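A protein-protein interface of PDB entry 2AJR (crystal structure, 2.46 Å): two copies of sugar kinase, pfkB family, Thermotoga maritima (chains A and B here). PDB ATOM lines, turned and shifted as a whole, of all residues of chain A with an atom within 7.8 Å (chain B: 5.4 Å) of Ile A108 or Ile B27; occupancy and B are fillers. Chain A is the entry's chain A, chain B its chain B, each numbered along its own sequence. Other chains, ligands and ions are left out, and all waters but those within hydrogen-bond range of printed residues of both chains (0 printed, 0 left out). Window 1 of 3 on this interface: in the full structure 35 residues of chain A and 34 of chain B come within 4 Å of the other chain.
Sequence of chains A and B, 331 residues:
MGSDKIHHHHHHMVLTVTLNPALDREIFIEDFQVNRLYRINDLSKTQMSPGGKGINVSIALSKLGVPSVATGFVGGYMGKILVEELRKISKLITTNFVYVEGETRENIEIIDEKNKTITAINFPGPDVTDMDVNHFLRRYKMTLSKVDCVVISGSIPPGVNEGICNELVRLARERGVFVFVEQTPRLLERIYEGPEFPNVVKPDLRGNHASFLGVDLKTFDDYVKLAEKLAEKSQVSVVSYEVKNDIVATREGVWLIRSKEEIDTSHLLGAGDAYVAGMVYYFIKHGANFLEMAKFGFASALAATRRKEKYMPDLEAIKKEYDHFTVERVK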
ATOM      1  N   ALA A  22      -6.319 -10.081   4.934  1.00  0.00           N
ATOM      2  CA  ALA A  22      -7.288 -10.358   3.880  1.00  0.00           C
ATOM      3  C   ALA A  22      -8.245 -11.467   4.285  1.00  0.00           C
ATOM      4  O   ALA A  22      -7.903 -12.308   5.098  1.00  0.00           O
ATOM      5  CB  ALA A  22      -6.574 -10.706   2.592  1.00  0.00           C
ATOM      6  N   LEU A  23      -9.458 -11.428   3.746  1.00  0.00           N
ATOM      7  CA  LEU A  23     -10.311 -12.600   3.671  1.00  0.00           C
ATOM      8  C   LEU A  23      -9.976 -13.340   2.385  1.00  0.00           C
ATOM      9  O   LEU A  23     -10.042 -12.773   1.308  1.00  0.00           O
ATOM     10  CB  LEU A  23     -11.778 -12.196   3.642  1.00  0.00           C
ATOM     11  CG  LEU A  23     -12.298 -11.739   4.992  1.00  0.00           C
ATOM     12  CD1 LEU A  23     -13.588 -10.968   4.824  1.00  0.00           C
ATOM     13  CD2 LEU A  23     -12.491 -12.953   5.876  1.00  0.00           C
ATOM     14  N   ASP A  24      -9.600 -14.600   2.499  1.00  0.00           N
ATOM     15  CA  ASP A  24      -9.266 -15.403   1.344  1.00  0.00           C
ATOM     16  C   ASP A  24     -10.516 -16.142   0.925  1.00  0.00           C
ATOM     17  O   ASP A  24     -11.084 -16.902   1.712  1.00  0.00           O
ATOM     18  CB  ASP A  24      -8.164 -16.410   1.679  1.00  0.00           C
ATOM     19  CG  ASP A  24      -6.787 -15.798   1.661  1.00  0.00           C
ATOM     20  OD1 ASP A  24      -6.492 -15.026   0.709  1.00  0.00           O
ATOM     21  OD2 ASP A  24      -5.992 -16.093   2.597  1.00  0.00           O
ATOM     22  N   ARG A  25     -10.969 -15.894  -0.298  1.00  0.00           N
ATOM     23  CA  ARG A  25     -12.006 -16.704  -0.897  1.00  0.00           C
ATOM     24  C   ARG A  25     -11.393 -17.687  -1.876  1.00  0.00           C
ATOM     25  O   ARG A  25     -10.998 -17.311  -2.983  1.00  0.00           O
ATOM     26  CB  ARG A  25     -13.035 -15.847  -1.616  1.00  0.00           C
ATOM     27  CG  ARG A  25     -14.141 -16.721  -2.271  1.00  0.00           C
ATOM     28  CD  ARG A  25     -15.511 -16.084  -2.200  1.00  0.00           C
ATOM     29  NE  ARG A  25     -16.097 -16.146  -0.860  1.00  0.00           N
ATOM     30  CZ  ARG A  25     -16.666 -17.225  -0.317  1.00  0.00           C
ATOM     31  NH1 ARG A  25     -16.740 -18.377  -0.977  1.00  0.00           N
ATOM     32  NH2 ARG A  25     -17.170 -17.144   0.903  1.00  0.00           N
ATOM     33  N   GLU A  26     -11.326 -18.949  -1.460  1.00  0.00           N
ATOM     34  CA  GLU A  26     -10.836 -20.039  -2.305  1.00  0.00           C
ATOM     35  C   GLU A  26     -12.005 -20.699  -3.046  1.00  0.00           C
ATOM     36  O   GLU A  26     -13.062 -20.979  -2.484  1.00  0.00           O
ATOM     37  CB  GLU A  26     -10.089 -21.080  -1.463  1.00  0.00           C
ATOM     38  CG  GLU A  26      -8.949 -20.546  -0.542  1.00  0.00           C
ATOM     39  CD  GLU A  26      -8.938 -21.228   0.870  1.00  0.00           C
ATOM     40  OE1 GLU A  26      -8.442 -22.393   0.964  1.00  0.00           O
ATOM     41  OE2 GLU A  26      -9.428 -20.590   1.873  1.00  0.00           O
ATOM     42  N   ILE A  27     -11.807 -20.937  -4.327  1.00  0.00           N
ATOM     43  CA  ILE A  27     -12.823 -21.527  -5.174  1.00  0.00           C
ATOM     44  C   ILE A  27     -12.115 -22.625  -5.942  1.00  0.00           C
ATOM     45  O   ILE A  27     -11.051 -22.386  -6.506  1.00  0.00           O
ATOM     46  CB  ILE A  27     -13.386 -20.487  -6.161  1.00  0.00           C
ATOM     47  CG1 ILE A  27     -13.730 -19.187  -5.430  1.00  0.00           C
ATOM     48  CG2 ILE A  27     -14.612 -21.035  -6.892  1.00  0.00           C
ATOM     49  CD1 ILE A  27     -13.823 -17.996  -6.341  1.00  0.00           C
ATOM     50  N   ARG A 105      -9.376  -6.102   2.616  1.00  0.00           N
ATOM     51  CA  ARG A 105      -9.460  -6.670   1.282  1.00  0.00           C
ATOM     52  C   ARG A 105      -9.979  -8.101   1.271  1.00  0.00           C
ATOM     53  O   ARG A 105      -9.771  -8.851   2.209  1.00  0.00           O
ATOM     54  CB  ARG A 105      -8.099  -6.601   0.603  1.00  0.00           C
ATOM     55  CG  ARG A 105      -7.030  -7.517   1.191  1.00  0.00           C
ATOM     56  CD  ARG A 105      -5.723  -6.818   1.148  1.00  0.00           C
ATOM     57  NE  ARG A 105      -4.600  -7.586   1.678  1.00  0.00           N
ATOM     58  CZ  ARG A 105      -3.687  -8.212   0.937  1.00  0.00           C
ATOM     59  NH1 ARG A 105      -3.760  -8.202  -0.382  1.00  0.00           N
ATOM     60  NH2 ARG A 105      -2.707  -8.879   1.523  1.00  0.00           N
ATOM     61  N   GLU A 106     -10.687  -8.473   0.219  1.00  0.00           N
ATOM     62  CA  GLU A 106     -11.009  -9.871   0.008  1.00  0.00           C
ATOM     63  C   GLU A 106     -10.203 -10.289  -1.207  1.00  0.00           C
ATOM     64  O   GLU A 106     -10.376  -9.718  -2.276  1.00  0.00           O
ATOM     65  CB  GLU A 106     -12.506 -10.097  -0.213  1.00  0.00           C
ATOM     66  CG  GLU A 106     -12.883 -11.599  -0.391  1.00  0.00           C
ATOM     67  CD  GLU A 106     -14.387 -11.882  -0.670  1.00  0.00           C
ATOM     68  OE1 GLU A 106     -15.036 -11.085  -1.384  1.00  0.00           O
ATOM     69  OE2 GLU A 106     -14.910 -12.928  -0.199  1.00  0.00           O
ATOM     70  N   ASN A 107      -9.295 -11.252  -1.030  1.00  0.00           N
ATOM     71  CA  ASN A 107      -8.553 -11.835  -2.143  1.00  0.00           C
ATOM     72  C   ASN A 107      -9.243 -13.080  -2.657  1.00  0.00           C
ATOM     73  O   ASN A 107      -9.967 -13.755  -1.918  1.00  0.00           O
ATOM     74  CB  ASN A 107      -7.116 -12.164  -1.733  1.00  0.00           C
ATOM     75  CG  ASN A 107      -6.309 -10.922  -1.429  1.00  0.00           C
ATOM     76  OD1 ASN A 107      -6.715  -9.804  -1.757  1.00  0.00           O
ATOM     77  ND2 ASN A 107      -5.181 -11.104  -0.781  1.00  0.00           N
ATOM     78  N   ILE A 108      -9.000 -13.386  -3.926  1.00  0.00           N
ATOM     79  CA  ILE A 108      -9.648 -14.516  -4.588  1.00  0.00           C
ATOM     80  C   ILE A 108      -8.602 -15.467  -5.159  1.00  0.00           C
ATOM     81  O   ILE A 108      -7.694 -15.042  -5.854  1.00  0.00           O
ATOM     82  CB  ILE A 108     -10.603 -14.021  -5.698  1.00  0.00           C
ATOM     83  CG1 ILE A 108     -11.782 -13.264  -5.058  1.00  0.00           C
ATOM     84  CG2 ILE A 108     -11.091 -15.180  -6.535  1.00  0.00           C
ATOM     85  CD1 ILE A 108     -12.639 -12.507  -6.019  1.00  0.00           C
ATOM     86  N   GLU A 109      -8.718 -16.748  -4.825  1.00  0.00           N
ATOM     87  CA  GLU A 109      -7.821 -17.775  -5.342  1.00  0.00           C
ATOM     88  C   GLU A 109      -8.671 -18.875  -5.969  1.00  0.00           C
ATOM     89  O   GLU A 109      -9.485 -19.493  -5.298  1.00  0.00           O
ATOM     90  CB  GLU A 109      -6.929 -18.339  -4.233  1.00  0.00           C
ATOM     91  CG  GLU A 109      -6.067 -17.289  -3.477  1.00  0.00           C
ATOM     92  CD  GLU A 109      -6.747 -16.746  -2.214  1.00  0.00           C
ATOM     93  OE1 GLU A 109      -7.673 -17.407  -1.705  1.00  0.00           O
ATOM     94  OE2 GLU A 109      -6.365 -15.665  -1.725  1.00  0.00           O
ATOM     95  N   ILE A 110      -8.513 -19.063  -7.271  1.00  0.00           N
ATOM     96  CA  ILE A 110      -9.186 -20.122  -8.006  1.00  0.00           C
ATOM     97  C   ILE A 110      -8.174 -21.246  -8.237  1.00  0.00           C
ATOM     98  O   ILE A 110      -7.114 -21.034  -8.816  1.00  0.00           O
ATOM     99  CB  ILE A 110      -9.745 -19.591  -9.340  1.00  0.00           C
ATOM    100  CG1 ILE A 110     -10.706 -18.422  -9.069  1.00  0.00           C
ATOM    101  CG2 ILE A 110     -10.450 -20.717 -10.116  1.00  0.00           C
ATOM    102  CD1 ILE A 110     -10.954 -17.520 -10.246  1.00  0.00           C
ATOM    103  N   ILE A 111      -8.487 -22.436  -7.743  1.00  0.00           N
ATOM    104  CA  ILE A 111      -7.534 -23.543  -7.728  1.00  0.00           C
ATOM    105  C   ILE A 111      -8.088 -24.648  -8.587  1.00  0.00           C
ATOM    106  O   ILE A 111      -9.200 -25.109  -8.346  1.00  0.00           O
ATOM    107  CB  ILE A 111      -7.284 -24.009  -6.302  1.00  0.00           C
ATOM    108  CG1 ILE A 111      -6.591 -22.868  -5.524  1.00  0.00           C
ATOM    109  CG2 ILE A 111      -6.439 -25.252  -6.287  1.00  0.00           C
ATOM    110  CD1 ILE A 111      -6.442 -23.099  -4.039  1.00  0.00           C
ATOM    111  N   ILE A 118      -3.271 -22.130 -10.090  1.00  0.00           N
ATOM    112  CA  ILE A 118      -3.822 -21.133  -9.176  1.00  0.00           C
ATOM    113  C   ILE A 118      -3.889 -19.835  -9.997  1.00  0.00           C
ATOM    114  O   ILE A 118      -2.867 -19.337 -10.517  1.00  0.00           O
ATOM    115  CB  ILE A 118      -2.927 -20.858  -7.895  1.00  0.00           C
ATOM    116  CG1 ILE A 118      -2.304 -22.133  -7.342  1.00  0.00           C
ATOM    117  CG2 ILE A 118      -3.736 -20.228  -6.744  1.00  0.00           C
ATOM    118  CD1 ILE A 118      -1.438 -21.919  -6.028  1.00  0.00           C
ATOM    119  N   THR A 119      -5.094 -19.308 -10.144  1.00  0.00           N
ATOM    120  CA  THR A 119      -5.302 -17.971 -10.662  1.00  0.00           C
ATOM    121  C   THR A 119      -5.671 -17.162  -9.425  1.00  0.00           C
ATOM    122  O   THR A 119      -6.650 -17.488  -8.743  1.00  0.00           O
ATOM    123  CB  THR A 119      -6.424 -17.977 -11.669  1.00  0.00           C
ATOM    124  OG1 THR A 119      -6.174 -19.020 -12.602  1.00  0.00           O
ATOM    125  CG2 THR A 119      -6.532 -16.653 -12.392  1.00  0.00           C
ATOM    126  N   ALA A 120      -4.870 -16.148  -9.102  1.00  0.00           N
ATOM    127  CA  ALA A 120      -5.066 -15.405  -7.845  1.00  0.00           C
ATOM    128  C   ALA A 120      -5.264 -13.936  -8.136  1.00  0.00           C
ATOM    129  O   ALA A 120      -4.615 -13.382  -9.022  1.00  0.00           O
ATOM    130  CB  ALA A 120      -3.888 -15.611  -6.896  1.00  0.00           C
ATOM    131  N   ILE A 121      -6.184 -13.316  -7.401  1.00  0.00           N
ATOM    132  CA  ILE A 121      -6.446 -11.894  -7.544  1.00  0.00           C
ATOM    133  C   ILE A 121      -6.292 -11.221  -6.180  1.00  0.00           C
ATOM    134  O   ILE A 121      -7.058 -11.500  -5.254  1.00  0.00           O
ATOM    135  CB  ILE A 121      -7.848 -11.615  -8.095  1.00  0.00           C
ATOM    136  CG1 ILE A 121      -8.088 -12.401  -9.386  1.00  0.00           C
ATOM    137  CG2 ILE A 121      -8.001 -10.129  -8.341  1.00  0.00           C
ATOM    138  CD1 ILE A 121      -9.505 -12.353  -9.883  1.00  0.00           C
ATOM    139  N   ASN A 122      -5.293 -10.350  -6.067  1.00  0.00           N
ATOM    140  CA  ASN A 122      -4.973  -9.722  -4.794  1.00  0.00           C
ATOM    141  C   ASN A 122      -5.286  -8.255  -4.800  1.00  0.00           C
ATOM    142  O   ASN A 122      -4.739  -7.463  -5.568  1.00  0.00           O
ATOM    143  CB  ASN A 122      -3.516  -9.966  -4.410  1.00  0.00           C
ATOM    144  CG  ASN A 122      -3.261 -11.422  -4.022  1.00  0.00           C
ATOM    145  OD1 ASN A 122      -4.190 -12.173  -3.753  1.00  0.00           O
ATOM    146  ND2 ASN A 122      -2.011 -11.816  -4.008  1.00  0.00           N
ATOM    147  N   PHE A 123      -6.209  -7.912  -3.934  1.00  0.00           N
ATOM    148  CA  PHE A 123      -6.638  -6.551  -3.800  1.00  0.00           C
ATOM    149  C   PHE A 123      -5.697  -5.802  -2.881  1.00  0.00           C
ATOM    150  O   PHE A 123      -5.022  -6.392  -2.062  1.00  0.00           O
ATOM    151  CB  PHE A 123      -8.106  -6.528  -3.325  1.00  0.00           C
ATOM    152  CG  PHE A 123      -9.082  -6.717  -4.464  1.00  0.00           C
ATOM    153  CD1 PHE A 123      -9.248  -7.962  -5.047  1.00  0.00           C
ATOM    154  CD2 PHE A 123      -9.766  -5.633  -4.999  1.00  0.00           C
ATOM    155  CE1 PHE A 123     -10.117  -8.131  -6.111  1.00  0.00           C
ATOM    156  CE2 PHE A 123     -10.642  -5.802  -6.059  1.00  0.00           C
ATOM    157  CZ  PHE A 123     -10.804  -7.045  -6.624  1.00  0.00           C
ATOM    158  N   LEU A 269      -1.114 -22.298  -1.577  1.00  0.00           N
ATOM    159  CA  LEU A 269      -1.585 -21.107  -0.877  1.00  0.00           C
ATOM    160  C   LEU A 269      -1.308 -21.234   0.613  1.00  0.00           C
ATOM    161  O   LEU A 269      -1.806 -22.157   1.265  1.00  0.00           O
ATOM    162  CB  LEU A 269      -3.065 -20.868  -1.094  1.00  0.00           C
ATOM    163  CG  LEU A 269      -3.581 -19.605  -0.403  1.00  0.00           C
ATOM    164  CD1 LEU A 269      -2.992 -18.341  -1.056  1.00  0.00           C
ATOM    165  CD2 LEU A 269      -5.091 -19.593  -0.422  1.00  0.00           C
ATOM    166  N   ARG B  25     -19.525  -8.772  -7.339  1.00  0.00           N
ATOM    167  CA  ARG B  25     -18.123  -8.358  -7.202  1.00  0.00           C
ATOM    168  C   ARG B  25     -17.511  -8.306  -8.592  1.00  0.00           C
ATOM    169  O   ARG B  25     -17.200  -9.344  -9.170  1.00  0.00           O
ATOM    170  CB  ARG B  25     -17.359  -9.367  -6.358  1.00  0.00           C
ATOM    171  CG  ARG B  25     -15.937  -8.977  -6.017  1.00  0.00           C
ATOM    172  CD  ARG B  25     -15.830  -8.442  -4.619  1.00  0.00           C
ATOM    173  NE  ARG B  25     -14.521  -7.848  -4.396  1.00  0.00           N
ATOM    174  CZ  ARG B  25     -13.448  -8.513  -3.975  1.00  0.00           C
ATOM    175  NH1 ARG B  25     -13.505  -9.819  -3.722  1.00  0.00           N
ATOM    176  NH2 ARG B  25     -12.304  -7.861  -3.799  1.00  0.00           N
ATOM    177  N   GLU B  26     -17.357  -7.092  -9.111  1.00  0.00           N
ATOM    178  CA  GLU B  26     -16.821  -6.861 -10.447  1.00  0.00           C
ATOM    179  C   GLU B  26     -15.339  -6.548 -10.341  1.00  0.00           C
ATOM    180  O   GLU B  26     -14.933  -5.690  -9.560  1.00  0.00           O
ATOM    181  CB  GLU B  26     -17.516  -5.665 -11.100  1.00  0.00           C
ATOM    182  CG  GLU B  26     -19.008  -5.763 -11.184  1.00  0.00           C
ATOM    183  CD  GLU B  26     -19.684  -4.378 -11.240  1.00  0.00           C
ATOM    184  OE1 GLU B  26     -19.419  -3.616 -12.209  1.00  0.00           O
ATOM    185  OE2 GLU B  26     -20.484  -4.062 -10.311  1.00  0.00           O
ATOM    186  N   ILE B  27     -14.537  -7.239 -11.133  1.00  0.00           N
ATOM    187  CA  ILE B  27     -13.096  -7.120 -11.066  1.00  0.00           C
ATOM    188  C   ILE B  27     -12.646  -6.883 -12.476  1.00  0.00           C
ATOM    189  O   ILE B  27     -13.020  -7.642 -13.365  1.00  0.00           O
ATOM    190  CB  ILE B  27     -12.473  -8.395 -10.531  1.00  0.00           C
ATOM    191  CG1 ILE B  27     -13.067  -8.743  -9.154  1.00  0.00           C
ATOM    192  CG2 ILE B  27     -10.979  -8.264 -10.457  1.00  0.00           C
ATOM    193  CD1 ILE B  27     -12.707 -10.150  -8.669  1.00  0.00           C
ATOM    194  N   PHE B  28     -11.857  -5.827 -12.684  1.00  0.00           N
ATOM    195  CA  PHE B  28     -11.428  -5.405 -14.030  1.00  0.00           C
ATOM    196  C   PHE B  28      -9.973  -5.697 -14.265  1.00  0.00           C
ATOM    197  O   PHE B  28      -9.121  -5.023 -13.705  1.00  0.00           O
ATOM    198  CB  PHE B  28     -11.706  -3.917 -14.199  1.00  0.00           C
ATOM    199  CG  PHE B  28     -13.123  -3.595 -13.976  1.00  0.00           C
ATOM    200  CD1 PHE B  28     -14.088  -4.094 -14.845  1.00  0.00           C
ATOM    201  CD2 PHE B  28     -13.525  -2.906 -12.847  1.00  0.00           C
ATOM    202  CE1 PHE B  28     -15.424  -3.855 -14.624  1.00  0.00           C
ATOM    203  CE2 PHE B  28     -14.881  -2.653 -12.619  1.00  0.00           C
ATOM    204  CZ  PHE B  28     -15.827  -3.131 -13.505  1.00  0.00           C
ATOM    205  N   ILE B  29      -9.711  -6.715 -15.081  1.00  0.00           N
ATOM    206  CA  ILE B  29      -8.361  -7.160 -15.393  1.00  0.00           C
ATOM    207  C   ILE B  29      -8.217  -7.310 -16.903  1.00  0.00           C
ATOM    208  O   ILE B  29      -8.904  -8.106 -17.521  1.00  0.00           O
ATOM    209  CB  ILE B  29      -8.038  -8.518 -14.739  1.00  0.00           C
ATOM    210  CG1 ILE B  29      -8.208  -8.443 -13.216  1.00  0.00           C
ATOM    211  CG2 ILE B  29      -6.626  -8.928 -15.087  1.00  0.00           C
ATOM    212  CD1 ILE B  29      -8.059  -9.792 -12.491  1.00  0.00           C
ATOM    213  N   ILE B  40      -4.250  -6.055  -8.120  1.00  0.00           N
ATOM    214  CA  ILE B  40      -5.102  -4.935  -8.467  1.00  0.00           C
ATOM    215  C   ILE B  40      -4.481  -3.629  -7.962  1.00  0.00           C
ATOM    216  O   ILE B  40      -3.822  -3.611  -6.916  1.00  0.00           O
ATOM    217  CB  ILE B  40      -6.493  -5.108  -7.838  1.00  0.00           C
ATOM    218  CG1 ILE B  40      -7.185  -6.369  -8.399  1.00  0.00           C
ATOM    219  CG2 ILE B  40      -7.382  -3.874  -8.085  1.00  0.00           C
ATOM    220  CD1 ILE B  40      -7.232  -6.486  -9.954  1.00  0.00           C
ATOM    221  N   ILE B 108     -19.065 -13.364  -8.546  1.00  0.00           N
ATOM    222  CA  ILE B 108     -17.835 -12.749  -9.028  1.00  0.00           C
ATOM    223  C   ILE B 108     -17.875 -12.653 -10.534  1.00  0.00           C
ATOM    224  O   ILE B 108     -18.172 -13.634 -11.228  1.00  0.00           O
ATOM    225  CB  ILE B 108     -16.613 -13.576  -8.617  1.00  0.00           C
ATOM    226  CG1 ILE B 108     -16.544 -13.665  -7.087  1.00  0.00           C
ATOM    227  CG2 ILE B 108     -15.334 -12.976  -9.184  1.00  0.00           C
ATOM    228  CD1 ILE B 108     -15.520 -14.648  -6.573  1.00  0.00           C
ATOM    229  N   GLU B 109     -17.587 -11.461 -11.038  1.00  0.00           N
ATOM    230  CA  GLU B 109     -17.494 -11.238 -12.470  1.00  0.00           C
ATOM    231  C   GLU B 109     -16.126 -10.629 -12.827  1.00  0.00           C
ATOM    232  O   GLU B 109     -15.824  -9.501 -12.458  1.00  0.00           O
ATOM    233  CB  GLU B 109     -18.635 -10.331 -12.938  1.00  0.00           C
ATOM    234  CG  GLU B 109     -20.054 -10.868 -12.629  1.00  0.00           C
ATOM    235  CD  GLU B 109     -20.665 -10.299 -11.333  1.00  0.00           C
ATOM    236  OE1 GLU B 109     -20.290  -9.180 -10.911  1.00  0.00           O
ATOM    237  OE2 GLU B 109     -21.536 -10.973 -10.734  1.00  0.00           O
ATOM    238  N   ILE B 110     -15.298 -11.386 -13.532  1.00  0.00           N
ATOM    239  CA  ILE B 110     -13.989 -10.909 -13.971  1.00  0.00           C
ATOM    240  C   ILE B 110     -14.131 -10.440 -15.401  1.00  0.00           C
ATOM    241  O   ILE B 110     -14.374 -11.234 -16.295  1.00  0.00           O
ATOM    242  CB  ILE B 110     -12.921 -11.990 -13.857  1.00  0.00           C
ATOM    243  CG1 ILE B 110     -12.769 -12.419 -12.381  1.00  0.00           C
ATOM    244  CG2 ILE B 110     -11.594 -11.474 -14.395  1.00  0.00           C
ATOM    245  CD1 ILE B 110     -12.392 -13.870 -12.172  1.00  0.00           C
ATOM    246  N   ILE B 111     -14.014  -9.129 -15.586  1.00  0.00           N
ATOM    247  CA  ILE B 111     -14.289  -8.476 -16.843  1.00  0.00           C
ATOM    248  C   ILE B 111     -12.993  -7.998 -17.503  1.00  0.00           C
ATOM    249  O   ILE B 111     -12.228  -7.250 -16.906  1.00  0.00           O
ATOM    250  CB  ILE B 111     -15.240  -7.303 -16.599  1.00  0.00           C
ATOM    251  CG1 ILE B 111     -16.621  -7.850 -16.199  1.00  0.00           C
ATOM    252  CG2 ILE B 111     -15.320  -6.411 -17.834  1.00  0.00           C
ATOM    253  CD1 ILE B 111     -17.567  -6.817 -15.670  1.00  0.00           C
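O of Asn A122 is in hydrogen-bond range of N of Ile B40. NH1 of Arg B25 lies within salt-bridge range of OE1 of Glu A106, at 3.1 Å.
The backbone carbonyl oxygen of Glu A109 lies within hydrogen-bond range of the backbone NH of Ile A27. The backbone carbonyl oxygen of Phe A123 sits at hydrogen-bond distance from the guanidinium group of Arg A105 (2.8 Å). O of Ile A27 sits at hydrogen-bond distance from N of Ile A111, 2.8 Å away. The backbone NH of Ile B27 lies within hydrogen-bond range of the backbone carbonyl oxygen of Glu B109 (2.9 Å). OD1 of Asn A122 sits at hydrogen-bond distance from ND2 of Asn A107 (3.3 Å). O of Arg B25 is in hydrogen-bond range of N of Glu B109 (2.8 Å).
Ile B108 touches Ile A27 (CD1 to CD1, 3.8 Å). CD1 of Ile A108 touches NH1 of Arg B25, at 3.6 Å. Ile B27 touches Ile A108 (CD1 to CD1, 3.5 Å). CD1 of Ile A108 touches CD1 of Ile B108 (3.6 Å). CD1 of Ile A121 touches CD1 of Ile B29, 3.9 Å away. Ile A121 touches Ile B40 (CG2 to CG1, 3.8 Å). Ile A121 touches Ile B110. Arg B25 touches Phe A123. Phe A123 touches Ile B27.
Ile A108 touches just these residues of chain B: Arg B25, Ile B27 and Ile B108. Of the printed residues of chain A, Ile B27 touches Ile A108 and Phe A123. Of the printed residues of chain A, Ile B40 touches Ile A121 and Asn A122. Printed residues of chain A within 4 Å of Ile B108: Ile A27 and Ile A108. The nearest printed residue of chain B that does not touch Ile A108 is Ile B110 (5.9 Å). The nearest residue of chain A that does not touch Ile B27 is Ile A121 (4.1 Å).
Hydrophobic or aromatic side chains of chain B that line the printed part of chain A: Ile B27, Ile B29, Ile B40, Ile B108 and Ile B110. Printed residues of chain A that touch a printed residue of chain B: Ile A27, Glu A106, Ile A108, Ile A121, Asn A122 and Phe A123.
Ile A27 touches Ile B108, and with the chains exchanged Ile A108 touches Ile B27. Ile A108 touches Arg B25, but with the chains exchanged Arg A25 does not touch Ile B108 (4.6 Å). Ile B108 touches its own counterpart, Ile A108. Positions printed for both chains: 25, 26, 27, 108, 109, 110 and 111. Of the 11 pairs that touch across the chains among the printed residues, 3 have their exchanged pair printed and touching as well.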
